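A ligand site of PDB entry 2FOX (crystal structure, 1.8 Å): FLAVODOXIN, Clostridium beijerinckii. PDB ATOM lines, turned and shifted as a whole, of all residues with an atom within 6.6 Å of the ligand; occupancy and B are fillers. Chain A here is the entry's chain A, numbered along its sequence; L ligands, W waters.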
ATOM      1  N   TRP A   6      11.546  17.441   8.039  1.00  0.00           N
ATOM      2  CA  TRP A   6      11.230  18.724   8.641  1.00  0.00           C
ATOM      3  C   TRP A   6       9.716  18.623   8.920  1.00  0.00           C
ATOM      4  O   TRP A   6       8.966  18.110   8.078  1.00  0.00           O
ATOM      5  CB  TRP A   6      11.496  19.917   7.708  1.00  0.00           C
ATOM      6  CG  TRP A   6      11.225  21.231   8.425  1.00  0.00           C
ATOM      7  CD1 TRP A   6      12.090  21.905   9.250  1.00  0.00           C
ATOM      8  CD2 TRP A   6       9.968  21.934   8.500  1.00  0.00           C
ATOM      9  NE1 TRP A   6      11.446  22.961   9.857  1.00  0.00           N
ATOM     10  CE2 TRP A   6      10.143  23.006   9.414  1.00  0.00           C
ATOM     11  CE3 TRP A   6       8.708  21.763   7.895  1.00  0.00           C
ATOM     12  CZ2 TRP A   6       9.108  23.903   9.743  1.00  0.00           C
ATOM     13  CZ3 TRP A   6       7.673  22.660   8.224  1.00  0.00           C
ATOM     14  CH2 TRP A   6       7.885  23.717   9.141  1.00  0.00           C
ATOM     15  N   SER A   7       9.294  19.080  10.094  1.00  0.00           N
ATOM     16  CA  SER A   7       7.872  19.059  10.458  1.00  0.00           C
ATOM     17  C   SER A   7       7.561  20.306  11.293  1.00  0.00           C
ATOM     18  O   SER A   7       8.238  20.580  12.280  1.00  0.00           O
ATOM     19  CB  SER A   7       7.556  17.793  11.249  1.00  0.00           C
ATOM     20  OG  SER A   7       6.172  17.685  11.514  1.00  0.00           O
ATOM     21  N   GLY A   8       6.516  21.041  10.917  1.00  0.00           N
ATOM     22  CA  GLY A   8       6.145  22.247  11.621  1.00  0.00           C
ATOM     23  C   GLY A   8       5.203  22.047  12.772  1.00  0.00           C
ATOM     24  O   GLY A   8       5.254  22.772  13.753  1.00  0.00           O
ATOM     25  N   THR A   9       4.288  21.085  12.644  1.00  0.00           N
ATOM     26  CA  THR A   9       3.330  20.806  13.716  1.00  0.00           C
ATOM     27  C   THR A   9       3.436  19.367  14.239  1.00  0.00           C
ATOM     28  O   THR A   9       2.786  19.023  15.235  1.00  0.00           O
ATOM     29  CB  THR A   9       1.864  21.090  13.307  1.00  0.00           C
ATOM     30  OG1 THR A   9       1.392  20.066  12.401  1.00  0.00           O
ATOM     31  CG2 THR A   9       1.744  22.437  12.636  1.00  0.00           C
ATOM     32  N   GLY A  10       4.212  18.528  13.566  1.00  0.00           N
ATOM     33  CA  GLY A  10       4.378  17.163  14.020  1.00  0.00           C
ATOM     34  C   GLY A  10       3.779  16.097  13.122  1.00  0.00           C
ATOM     35  O   GLY A  10       3.952  14.911  13.401  1.00  0.00           O
ATOM     36  N   ASN A  11       3.110  16.482  12.045  1.00  0.00           N
ATOM     37  CA  ASN A  11       2.481  15.504  11.162  1.00  0.00           C
ATOM     38  C   ASN A  11       3.515  14.679  10.377  1.00  0.00           C
ATOM     39  O   ASN A  11       3.464  13.445  10.386  1.00  0.00           O
ATOM     40  CB  ASN A  11       1.474  16.173  10.216  1.00  0.00           C
ATOM     41  CG  ASN A  11       0.298  16.759  10.958  1.00  0.00           C
ATOM     42  OD1 ASN A  11      -0.384  17.651  10.452  1.00  0.00           O
ATOM     43  ND2 ASN A  11       0.063  16.286  12.169  1.00  0.00           N
ATOM     44  N   THR A  12       4.451  15.357   9.722  1.00  0.00           N
ATOM     45  CA  THR A  12       5.514  14.663   8.988  1.00  0.00           C
ATOM     46  C   THR A  12       6.441  13.916   9.964  1.00  0.00           C
ATOM     47  O   THR A  12       6.949  12.838   9.644  1.00  0.00           O
ATOM     48  CB  THR A  12       6.314  15.661   8.107  1.00  0.00           C
ATOM     49  OG1 THR A  12       5.400  16.306   7.217  1.00  0.00           O
ATOM     50  CG2 THR A  12       7.351  14.935   7.279  1.00  0.00           C
ATOM     51  N   GLU A  13       6.602  14.442  11.185  1.00  0.00           N
ATOM     52  CA  GLU A  13       7.429  13.802  12.203  1.00  0.00           C
ATOM     53  C   GLU A  13       6.828  12.437  12.564  1.00  0.00           C
ATOM     54  O   GLU A  13       7.546  11.440  12.683  1.00  0.00           O
ATOM     55  CB  GLU A  13       7.544  14.661  13.453  1.00  0.00           C
ATOM     56  CG  GLU A  13       8.466  14.079  14.533  1.00  0.00           C
ATOM     57  CD  GLU A  13       8.543  14.930  15.808  1.00  0.00           C
ATOM     58  OE1 GLU A  13       7.862  15.984  15.901  1.00  0.00           O
ATOM     59  OE2 GLU A  13       9.279  14.539  16.727  1.00  0.00           O
ATOM     60  N   CYS A  53       9.158  16.130   4.139  1.00  0.00           N
ATOM     61  CA  CYS A  53       8.857  17.532   4.437  1.00  0.00           C
ATOM     62  C   CYS A  53       7.418  17.807   4.041  1.00  0.00           C
ATOM     63  O   CYS A  53       6.963  17.370   2.982  1.00  0.00           O
ATOM     64  CB  CYS A  53       9.775  18.467   3.635  1.00  0.00           C
ATOM     65  SG  CYS A  53       9.595  20.243   4.005  1.00  0.00           S
ATOM     66  N   SER A  54       6.709  18.536   4.885  1.00  0.00           N
ATOM     67  CA  SER A  54       5.332  18.907   4.612  1.00  0.00           C
ATOM     68  C   SER A  54       5.244  19.978   3.524  1.00  0.00           C
ATOM     69  O   SER A  54       6.243  20.621   3.184  1.00  0.00           O
ATOM     70  CB  SER A  54       4.698  19.453   5.892  1.00  0.00           C
ATOM     71  OG  SER A  54       5.551  20.383   6.507  1.00  0.00           O
ATOM     72  N   ALA A  55       4.047  20.141   2.964  1.00  0.00           N
ATOM     73  CA  ALA A  55       3.807  21.156   1.944  1.00  0.00           C
ATOM     74  C   ALA A  55       3.782  22.506   2.658  1.00  0.00           C
ATOM     75  O   ALA A  55       3.045  22.694   3.640  1.00  0.00           O
ATOM     76  CB  ALA A  55       2.491  20.880   1.228  1.00  0.00           C
ATOM     77  N   MET A  56       4.664  23.417   2.235  1.00  0.00           N
ATOM     78  CA  MET A  56       4.768  24.740   2.847  1.00  0.00           C
ATOM     79  C   MET A  56       4.623  25.869   1.816  1.00  0.00           C
ATOM     80  O   MET A  56       4.490  25.616   0.620  1.00  0.00           O
ATOM     81  CB  MET A  56       6.079  24.863   3.614  1.00  0.00           C
ATOM     82  CG  MET A  56       6.105  24.043   4.874  1.00  0.00           C
ATOM     83  SD  MET A  56       4.886  24.587   6.097  1.00  0.00           S
ATOM     84  CE  MET A  56       5.668  25.942   6.743  1.00  0.00           C
ATOM     85  N   GLY A  57       4.620  27.117   2.301  1.00  0.00           N
ATOM     86  CA  GLY A  57       4.456  28.265   1.433  1.00  0.00           C
ATOM     87  C   GLY A  57       3.309  28.024   0.477  1.00  0.00           C
ATOM     88  O   GLY A  57       2.217  27.609   0.883  1.00  0.00           O
ATOM     89  N   ASP A  58       3.531  28.273  -0.795  1.00  0.00           N
ATOM     90  CA  ASP A  58       2.517  28.002  -1.789  1.00  0.00           C
ATOM     91  C   ASP A  58       3.044  26.807  -2.587  1.00  0.00           C
ATOM     92  O   ASP A  58       3.685  26.969  -3.618  1.00  0.00           O
ATOM     93  CB  ASP A  58       2.265  29.217  -2.685  1.00  0.00           C
ATOM     94  CG  ASP A  58       1.102  29.006  -3.672  1.00  0.00           C
ATOM     95  OD1 ASP A  58       0.279  28.077  -3.487  1.00  0.00           O
ATOM     96  OD2 ASP A  58       1.012  29.795  -4.645  1.00  0.00           O
ATOM     97  N   GLU A  59       2.824  25.610  -2.035  1.00  0.00           N
ATOM     98  CA  GLU A  59       3.238  24.347  -2.648  1.00  0.00           C
ATOM     99  C   GLU A  59       4.739  24.226  -2.884  1.00  0.00           C
ATOM    100  O   GLU A  59       5.171  23.863  -3.974  1.00  0.00           O
ATOM    101  CB  GLU A  59       2.485  24.051  -3.961  1.00  0.00           C
ATOM    102  CG  GLU A  59       0.981  23.809  -3.837  1.00  0.00           C
ATOM    103  CD  GLU A  59       0.581  22.586  -3.004  1.00  0.00           C
ATOM    104  OE1 GLU A  59       1.369  21.627  -2.880  1.00  0.00           O
ATOM    105  OE2 GLU A  59      -0.551  22.562  -2.494  1.00  0.00           O
ATOM    106  N   VAL A  60       5.527  24.490  -1.846  1.00  0.00           N
ATOM    107  CA  VAL A  60       6.983  24.376  -1.925  1.00  0.00           C
ATOM    108  C   VAL A  60       7.532  23.676  -0.685  1.00  0.00           C
ATOM    109  O   VAL A  60       6.805  23.451   0.285  1.00  0.00           O
ATOM    110  CB  VAL A  60       7.655  25.789  -2.021  1.00  0.00           C
ATOM    111  CG1 VAL A  60       7.289  26.463  -3.355  1.00  0.00           C
ATOM    112  CG2 VAL A  60       7.264  26.649  -0.844  1.00  0.00           C
ATOM    113  N   GLY A  86       5.738  12.990   3.059  1.00  0.00           N
ATOM    114  CA  GLY A  86       5.349  14.239   3.696  1.00  0.00           C
ATOM    115  C   GLY A  86       3.854  14.434   3.856  1.00  0.00           C
ATOM    116  O   GLY A  86       3.047  13.840   3.138  1.00  0.00           O
ATOM    117  N   SER A  87       3.503  15.263   4.830  1.00  0.00           N
ATOM    118  CA  SER A  87       2.114  15.579   5.113  1.00  0.00           C
ATOM    119  C   SER A  87       1.710  16.857   4.361  1.00  0.00           C
ATOM    120  O   SER A  87       2.557  17.723   4.091  1.00  0.00           O
ATOM    121  CB  SER A  87       1.925  15.791   6.622  1.00  0.00           C
ATOM    122  OG  SER A  87       0.549  16.015   6.924  1.00  0.00           O
ATOM    123  N   TYR A  88       0.441  16.979   4.018  1.00  0.00           N
ATOM    124  CA  TYR A  88      -0.037  18.174   3.328  1.00  0.00           C
ATOM    125  C   TYR A  88      -1.428  18.543   3.857  1.00  0.00           C
ATOM    126  O   TYR A  88      -2.018  17.814   4.661  1.00  0.00           O
ATOM    127  CB  TYR A  88      -0.030  17.996   1.806  1.00  0.00           C
ATOM    128  CG  TYR A  88      -1.018  16.981   1.298  1.00  0.00           C
ATOM    129  CD1 TYR A  88      -0.748  15.615   1.358  1.00  0.00           C
ATOM    130  CD2 TYR A  88      -2.224  17.403   0.738  1.00  0.00           C
ATOM    131  CE1 TYR A  88      -1.657  14.687   0.872  1.00  0.00           C
ATOM    132  CE2 TYR A  88      -3.142  16.478   0.250  1.00  0.00           C
ATOM    133  CZ  TYR A  88      -2.858  15.121   0.317  1.00  0.00           C
ATOM    134  OH  TYR A  88      -3.757  14.194  -0.149  1.00  0.00           O
ATOM    135  N   GLY A  89      -1.926  19.708   3.452  1.00  0.00           N
ATOM    136  CA  GLY A  89      -3.204  20.156   3.961  1.00  0.00           C
ATOM    137  C   GLY A  89      -4.318  20.280   2.936  1.00  0.00           C
ATOM    138  O   GLY A  89      -5.067  19.331   2.734  1.00  0.00           O
ATOM    139  N   TRP A  90      -4.363  21.417   2.257  1.00  0.00           N
ATOM    140  CA  TRP A  90      -5.434  21.676   1.280  1.00  0.00           C
ATOM    141  C   TRP A  90      -5.164  21.360  -0.188  1.00  0.00           C
ATOM    142  O   TRP A  90      -6.094  21.329  -0.980  1.00  0.00           O
ATOM    143  CB  TRP A  90      -5.859  23.133   1.407  1.00  0.00           C
ATOM    144  CG  TRP A  90      -4.707  24.110   1.298  1.00  0.00           C
ATOM    145  CD1 TRP A  90      -4.146  24.594   0.155  1.00  0.00           C
ATOM    146  CD2 TRP A  90      -4.000  24.704   2.378  1.00  0.00           C
ATOM    147  NE1 TRP A  90      -3.133  25.466   0.454  1.00  0.00           N
ATOM    148  CE2 TRP A  90      -3.020  25.558   1.821  1.00  0.00           C
ATOM    149  CE3 TRP A  90      -4.090  24.610   3.773  1.00  0.00           C
ATOM    150  CZ2 TRP A  90      -2.148  26.315   2.598  1.00  0.00           C
ATOM    151  CZ3 TRP A  90      -3.217  25.367   4.549  1.00  0.00           C
ATOM    152  CH2 TRP A  90      -2.262  26.211   3.965  1.00  0.00           C
ATOM    153  N   GLY A  91      -3.905  21.183  -0.543  1.00  0.00           N
ATOM    154  CA  GLY A  91      -3.573  20.922  -1.936  1.00  0.00           C
ATOM    155  C   GLY A  91      -3.783  19.480  -2.336  1.00  0.00           C
ATOM    156  O   GLY A  91      -4.406  18.705  -1.610  1.00  0.00           O
ATOM    157  N   ASP A  92      -3.275  19.123  -3.505  1.00  0.00           N
ATOM    158  CA  ASP A  92      -3.372  17.767  -4.002  1.00  0.00           C
ATOM    159  C   ASP A  92      -2.013  17.120  -4.311  1.00  0.00           C
ATOM    160  O   ASP A  92      -1.916  16.216  -5.145  1.00  0.00           O
ATOM    161  CB  ASP A  92      -4.357  17.645  -5.194  1.00  0.00           C
ATOM    162  CG  ASP A  92      -3.887  18.373  -6.456  1.00  0.00           C
ATOM    163  OD1 ASP A  92      -2.681  18.649  -6.611  1.00  0.00           O
ATOM    164  OD2 ASP A  92      -4.759  18.638  -7.317  1.00  0.00           O
ATOM    165  N   GLY A  93      -0.979  17.597  -3.628  1.00  0.00           N
ATOM    166  CA  GLY A  93       0.340  17.016  -3.800  1.00  0.00           C
ATOM    167  C   GLY A  93       1.299  17.678  -4.767  1.00  0.00           C
ATOM    168  O   GLY A  93       2.346  17.123  -5.061  1.00  0.00           O
ATOM    169  N   TRP A  95       3.478  20.090  -4.373  1.00  0.00           N
ATOM    170  CA  TRP A  95       4.833  20.235  -3.847  1.00  0.00           C
ATOM    171  C   TRP A  95       5.620  18.939  -3.959  1.00  0.00           C
ATOM    172  O   TRP A  95       6.815  18.963  -4.220  1.00  0.00           O
ATOM    173  CB  TRP A  95       4.835  20.771  -2.412  1.00  0.00           C
ATOM    174  CG  TRP A  95       5.048  19.733  -1.330  1.00  0.00           C
ATOM    175  CD1 TRP A  95       6.145  19.626  -0.510  1.00  0.00           C
ATOM    176  CD2 TRP A  95       4.138  18.706  -0.909  1.00  0.00           C
ATOM    177  NE1 TRP A  95       5.970  18.612   0.391  1.00  0.00           N
ATOM    178  CE2 TRP A  95       4.746  18.028   0.174  1.00  0.00           C
ATOM    179  CE3 TRP A  95       2.866  18.294  -1.329  1.00  0.00           C
ATOM    180  CZ2 TRP A  95       4.124  16.961   0.827  1.00  0.00           C
ATOM    181  CZ3 TRP A  95       2.252  17.244  -0.681  1.00  0.00           C
ATOM    182  CH2 TRP A  95       2.881  16.588   0.394  1.00  0.00           C
ATOM    183  N   VAL A 117       0.359  12.071   2.944  1.00  0.00           N
ATOM    184  CA  VAL A 117      -0.815  11.843   3.777  1.00  0.00           C
ATOM    185  C   VAL A 117      -1.361  13.204   4.163  1.00  0.00           C
ATOM    186  O   VAL A 117      -0.596  14.114   4.472  1.00  0.00           O
ATOM    187  CB  VAL A 117      -0.426  11.063   5.071  1.00  0.00           C
ATOM    188  CG1 VAL A 117      -1.580  11.018   6.054  1.00  0.00           C
ATOM    189  CG2 VAL A 117       0.029   9.645   4.698  1.00  0.00           C
ATOM    190  N   GLN A 118      -2.682  13.351   4.119  1.00  0.00           N
ATOM    191  CA  GLN A 118      -3.303  14.631   4.472  1.00  0.00           C
ATOM    192  C   GLN A 118      -3.399  14.779   5.987  1.00  0.00           C
ATOM    193  O   GLN A 118      -3.958  13.915   6.677  1.00  0.00           O
ATOM    194  CB  GLN A 118      -4.682  14.760   3.836  1.00  0.00           C
ATOM    195  CG  GLN A 118      -5.301  16.134   4.031  1.00  0.00           C
ATOM    196  CD  GLN A 118      -6.717  16.205   3.511  1.00  0.00           C
ATOM    197  OE1 GLN A 118      -6.960  16.600   2.369  1.00  0.00           O
ATOM    198  NE2 GLN A 118      -7.675  15.820   4.345  1.00  0.00           N
ATOM    199  N   ASN A 119      -2.844  15.880   6.496  1.00  0.00           N
ATOM    200  CA  ASN A 119      -2.848  16.196   7.920  1.00  0.00           C
ATOM    201  C   ASN A 119      -2.139  15.109   8.732  1.00  0.00           C
ATOM    202  O   ASN A 119      -1.154  14.546   8.264  1.00  0.00           O
ATOM    203  CB  ASN A 119      -4.287  16.444   8.406  1.00  0.00           C
ATOM    204  CG  ASN A 119      -5.030  17.460   7.513  1.00  0.00           C
ATOM    205  OD1 ASN A 119      -4.655  18.639   7.413  1.00  0.00           O
ATOM    206  ND2 ASN A 119      -6.060  16.989   6.818  1.00  0.00           N
ATOM    207  N   GLU A 120      -2.627  14.779   9.917  1.00  0.00           N
ATOM    208  CA  GLU A 120      -1.973  13.765  10.729  1.00  0.00           C
ATOM    209  C   GLU A 120      -2.292  12.353  10.239  1.00  0.00           C
ATOM    210  O   GLU A 120      -3.398  12.087   9.764  1.00  0.00           O
ATOM    211  CB  GLU A 120      -2.389  13.896  12.201  1.00  0.00           C
ATOM    212  CG  GLU A 120      -1.641  12.957  13.153  1.00  0.00           C
ATOM    213  CD  GLU A 120      -2.348  12.736  14.490  1.00  0.00           C
ATOM    214  OE1 GLU A 120      -3.567  12.443  14.482  1.00  0.00           O
ATOM    215  OE2 GLU A 120      -1.658  12.828  15.536  1.00  0.00           O
HETATM  216  N1  LIG L   1      -0.689  22.304   2.562  1.00  0.00           N
HETATM  217  C1  LIG L   1      -0.907  22.109   1.255  1.00  0.00           C
HETATM  218  O1  LIG L   1      -1.540  21.185   0.882  1.00  0.00           O
HETATM  219  N2  LIG L   1      -0.367  22.992   0.297  1.00  0.00           N
HETATM  220  C2  LIG L   1       0.322  24.155   0.600  1.00  0.00           C
HETATM  221  O2  LIG L   1       0.717  24.954  -0.261  1.00  0.00           O
HETATM  222  C3  LIG L   1       0.518  24.378   2.024  1.00  0.00           C
HETATM  223  N3  LIG L   1       1.121  25.460   2.410  1.00  0.00           N
HETATM  224  C4  LIG L   1       1.175  25.735   3.729  1.00  0.00           C
HETATM  225  C5  LIG L   1       1.729  26.968   4.152  1.00  0.00           C
HETATM  226  C6  LIG L   1       1.952  27.178   5.475  1.00  0.00           C
HETATM  227  C7  LIG L   1       2.644  28.416   5.963  1.00  0.00           C
HETATM  228  C8  LIG L   1       1.519  26.218   6.454  1.00  0.00           C
HETATM  229  C9  LIG L   1       1.718  26.436   7.933  1.00  0.00           C
HETATM  230  C10 LIG L   1       0.905  25.052   6.043  1.00  0.00           C
HETATM  231  C11 LIG L   1       0.746  24.781   4.696  1.00  0.00           C
HETATM  232  N4  LIG L   1       0.106  23.650   4.254  1.00  0.00           N
HETATM  233  C12 LIG L   1      -0.028  23.368   2.941  1.00  0.00           C
HETATM  234  C13 LIG L   1      -0.449  22.705   5.212  1.00  0.00           C
HETATM  235  C14 LIG L   1       0.570  21.690   5.745  1.00  0.00           C
HETATM  236  O3  LIG L   1       1.307  21.030   4.708  1.00  0.00           O
HETATM  237  C15 LIG L   1      -0.149  20.641   6.587  1.00  0.00           C
HETATM  238  O4  LIG L   1      -0.805  21.276   7.692  1.00  0.00           O
HETATM  239  C16 LIG L   1       0.730  19.473   7.092  1.00  0.00           C
HETATM  240  O5  LIG L   1      -0.086  18.520   7.780  1.00  0.00           O
HETATM  241  C17 LIG L   1       1.776  19.971   8.084  1.00  0.00           C
HETATM  242  O6  LIG L   1       2.697  18.945   8.456  1.00  0.00           O
HETATM  243  P1  LIG L   1       3.793  19.272   9.523  1.00  0.00           P
HETATM  244  O7  LIG L   1       4.519  20.463   9.129  1.00  0.00           O
HETATM  245  O8  LIG L   1       3.273  19.239  10.885  1.00  0.00           O
HETATM  246  O9  LIG L   1       4.700  18.077   9.298  1.00  0.00           O
HETATM  247  O   HOH W   1       3.595  23.069   9.363  1.00  0.00           O
HETATM  248  O   HOH W   2       0.829  23.180   9.184  1.00  0.00           O
HETATM  249  O   HOH W   3      -1.273  26.576  -1.374  1.00  0.00           O
HETATM  250  O   HOH W   4       5.839  28.660   4.657  1.00  0.00           O
HETATM  251  O   HOH W   5      -0.310  19.587  -1.617  1.00  0.00           O
HETATM  252  O   HOH W   6      -2.820  19.825   8.839  1.00  0.00           O
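A nitrogen (N3) of the ligand lies close to the backbone carbonyl oxygen (O) of Gly 57.
Merely in contact with the ligand: Tyr 88 (3.4 Å), Met 56 (3.6 Å), Asn 119 (3.6 Å), Asp 58 (3.8 Å) and Trp 6 (3.9 Å).
Hydrophobic or aromatic side chains within 4 Å of the ligand: Trp 6, Ala 55, Met 56, Tyr 88 and Trp 90.
Within 4 Å of the ligand: Trp 6, Ser 7, Gly 8, Thr 9, Gly 10, Asn 11, Thr 12, Ser 54, Ala 55, Met 56, Gly 57, Asp 58, Glu 59, Ser 87, Tyr 88, Gly 89, Trp 90, Gly 91 and Asn 119.
N of Thr 9 sits at hydrogen-bond distance from O8 of the ligand, 2.7 Å away.
O8 of the ligand lies within hydrogen-bond range of OG1 of Thr 9 (2.6 Å).
N of Ala 55 lies within hydrogen-bond range of O3 of the ligand (3.4 Å).
The backbone carbonyl oxygen of Ala 55 lies within hydrogen-bond range of an oxygen (O3) of the ligand, 2.6 Å away.
The side-chain hydroxyl of Ser 7 sits at hydrogen-bond distance from an oxygen (O9) of the ligand.
An oxygen (O5) of the ligand lies within hydrogen-bond range of the side-chain hydroxyl of Ser 87, at 2.7 Å.
N of Gly 8 sits at hydrogen-bond distance from O7 of the ligand (2.7 Å).
The backbone NH (N) of Gly 91 lies within hydrogen-bond range of an oxygen (O1) of the ligand (2.8 Å).
N of Thr 12 lies within hydrogen-bond range of O9 of the ligand.
OG1 of Thr 12 sits at hydrogen-bond distance from O9 of the ligand, at 2.8 Å.
OG of Ser 54 is in hydrogen-bond range of O7 of the ligand, at 2.8 Å.
N of Asn 11 sits at hydrogen-bond distance from O8 of the ligand (3.0 Å).
OD1 of Asn 11 lies within hydrogen-bond range of O5 of the ligand (2.8 Å).
The backbone NH (N) of Glu 59 sits at hydrogen-bond distance from an oxygen (O2) of the ligand.
OE2 of Glu 59 lies within hydrogen-bond range of N2 of the ligand (2.8 Å).
N of Gly 10 is in hydrogen-bond range of O8 of the ligand (2.9 Å).
N of Gly 89 sits at hydrogen-bond distance from O1 of the ligand, 3.0 Å away.
The backbone NH (N) of Trp 90 is in hydrogen-bond range of an oxygen (O1) of the ligand (3.1 Å).
Water W6 bridges the side-chain amide oxygen (OD1) of Asn 119 (2.6 Å) and an oxygen (O4) of the ligand (2.7 Å).
Water W3 lies within hydrogen-bond range of O2 of the ligand (2.8 Å), NE1 of Trp 90 (2.8 Å) and OD1 of Asp 58 (3.0 Å).
Water W5 lies within hydrogen-bond range of the backbone NH (N) of Gly 93, the side-chain carboxylate (OE1) of Glu 59 and an oxygen (O1) of the ligand.
N of Ala 55 sits at hydrogen-bond distance from O of Ser 87 (3.1 Å).
The side-chain hydroxyl (OG) of Ser 7 sits at hydrogen-bond distance from the backbone NH (N) of Asn 11, 3.3 Å away.
N of Gly 10 is in hydrogen-bond range of OG of Ser 7 (3.0 Å).
The backbone NH (N) of Ser 87 sits at hydrogen-bond distance from the side-chain hydroxyl (OG1) of Thr 12 (3.2 Å).
O of Asn 119 is in hydrogen-bond range of OG of Ser 87.
The side-chain hydroxyl (OG) of Ser 87 lies close to the backbone carbonyl oxygen (O) of Val 117 (3.3 Å).
The backbone NH (N) of Asn 119 is in hydrogen-bond range of the backbone carbonyl oxygen (O) of Tyr 88 (2.8 Å).
N of Tyr 88 sits at hydrogen-bond distance from O of Val 117 (3.1 Å).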
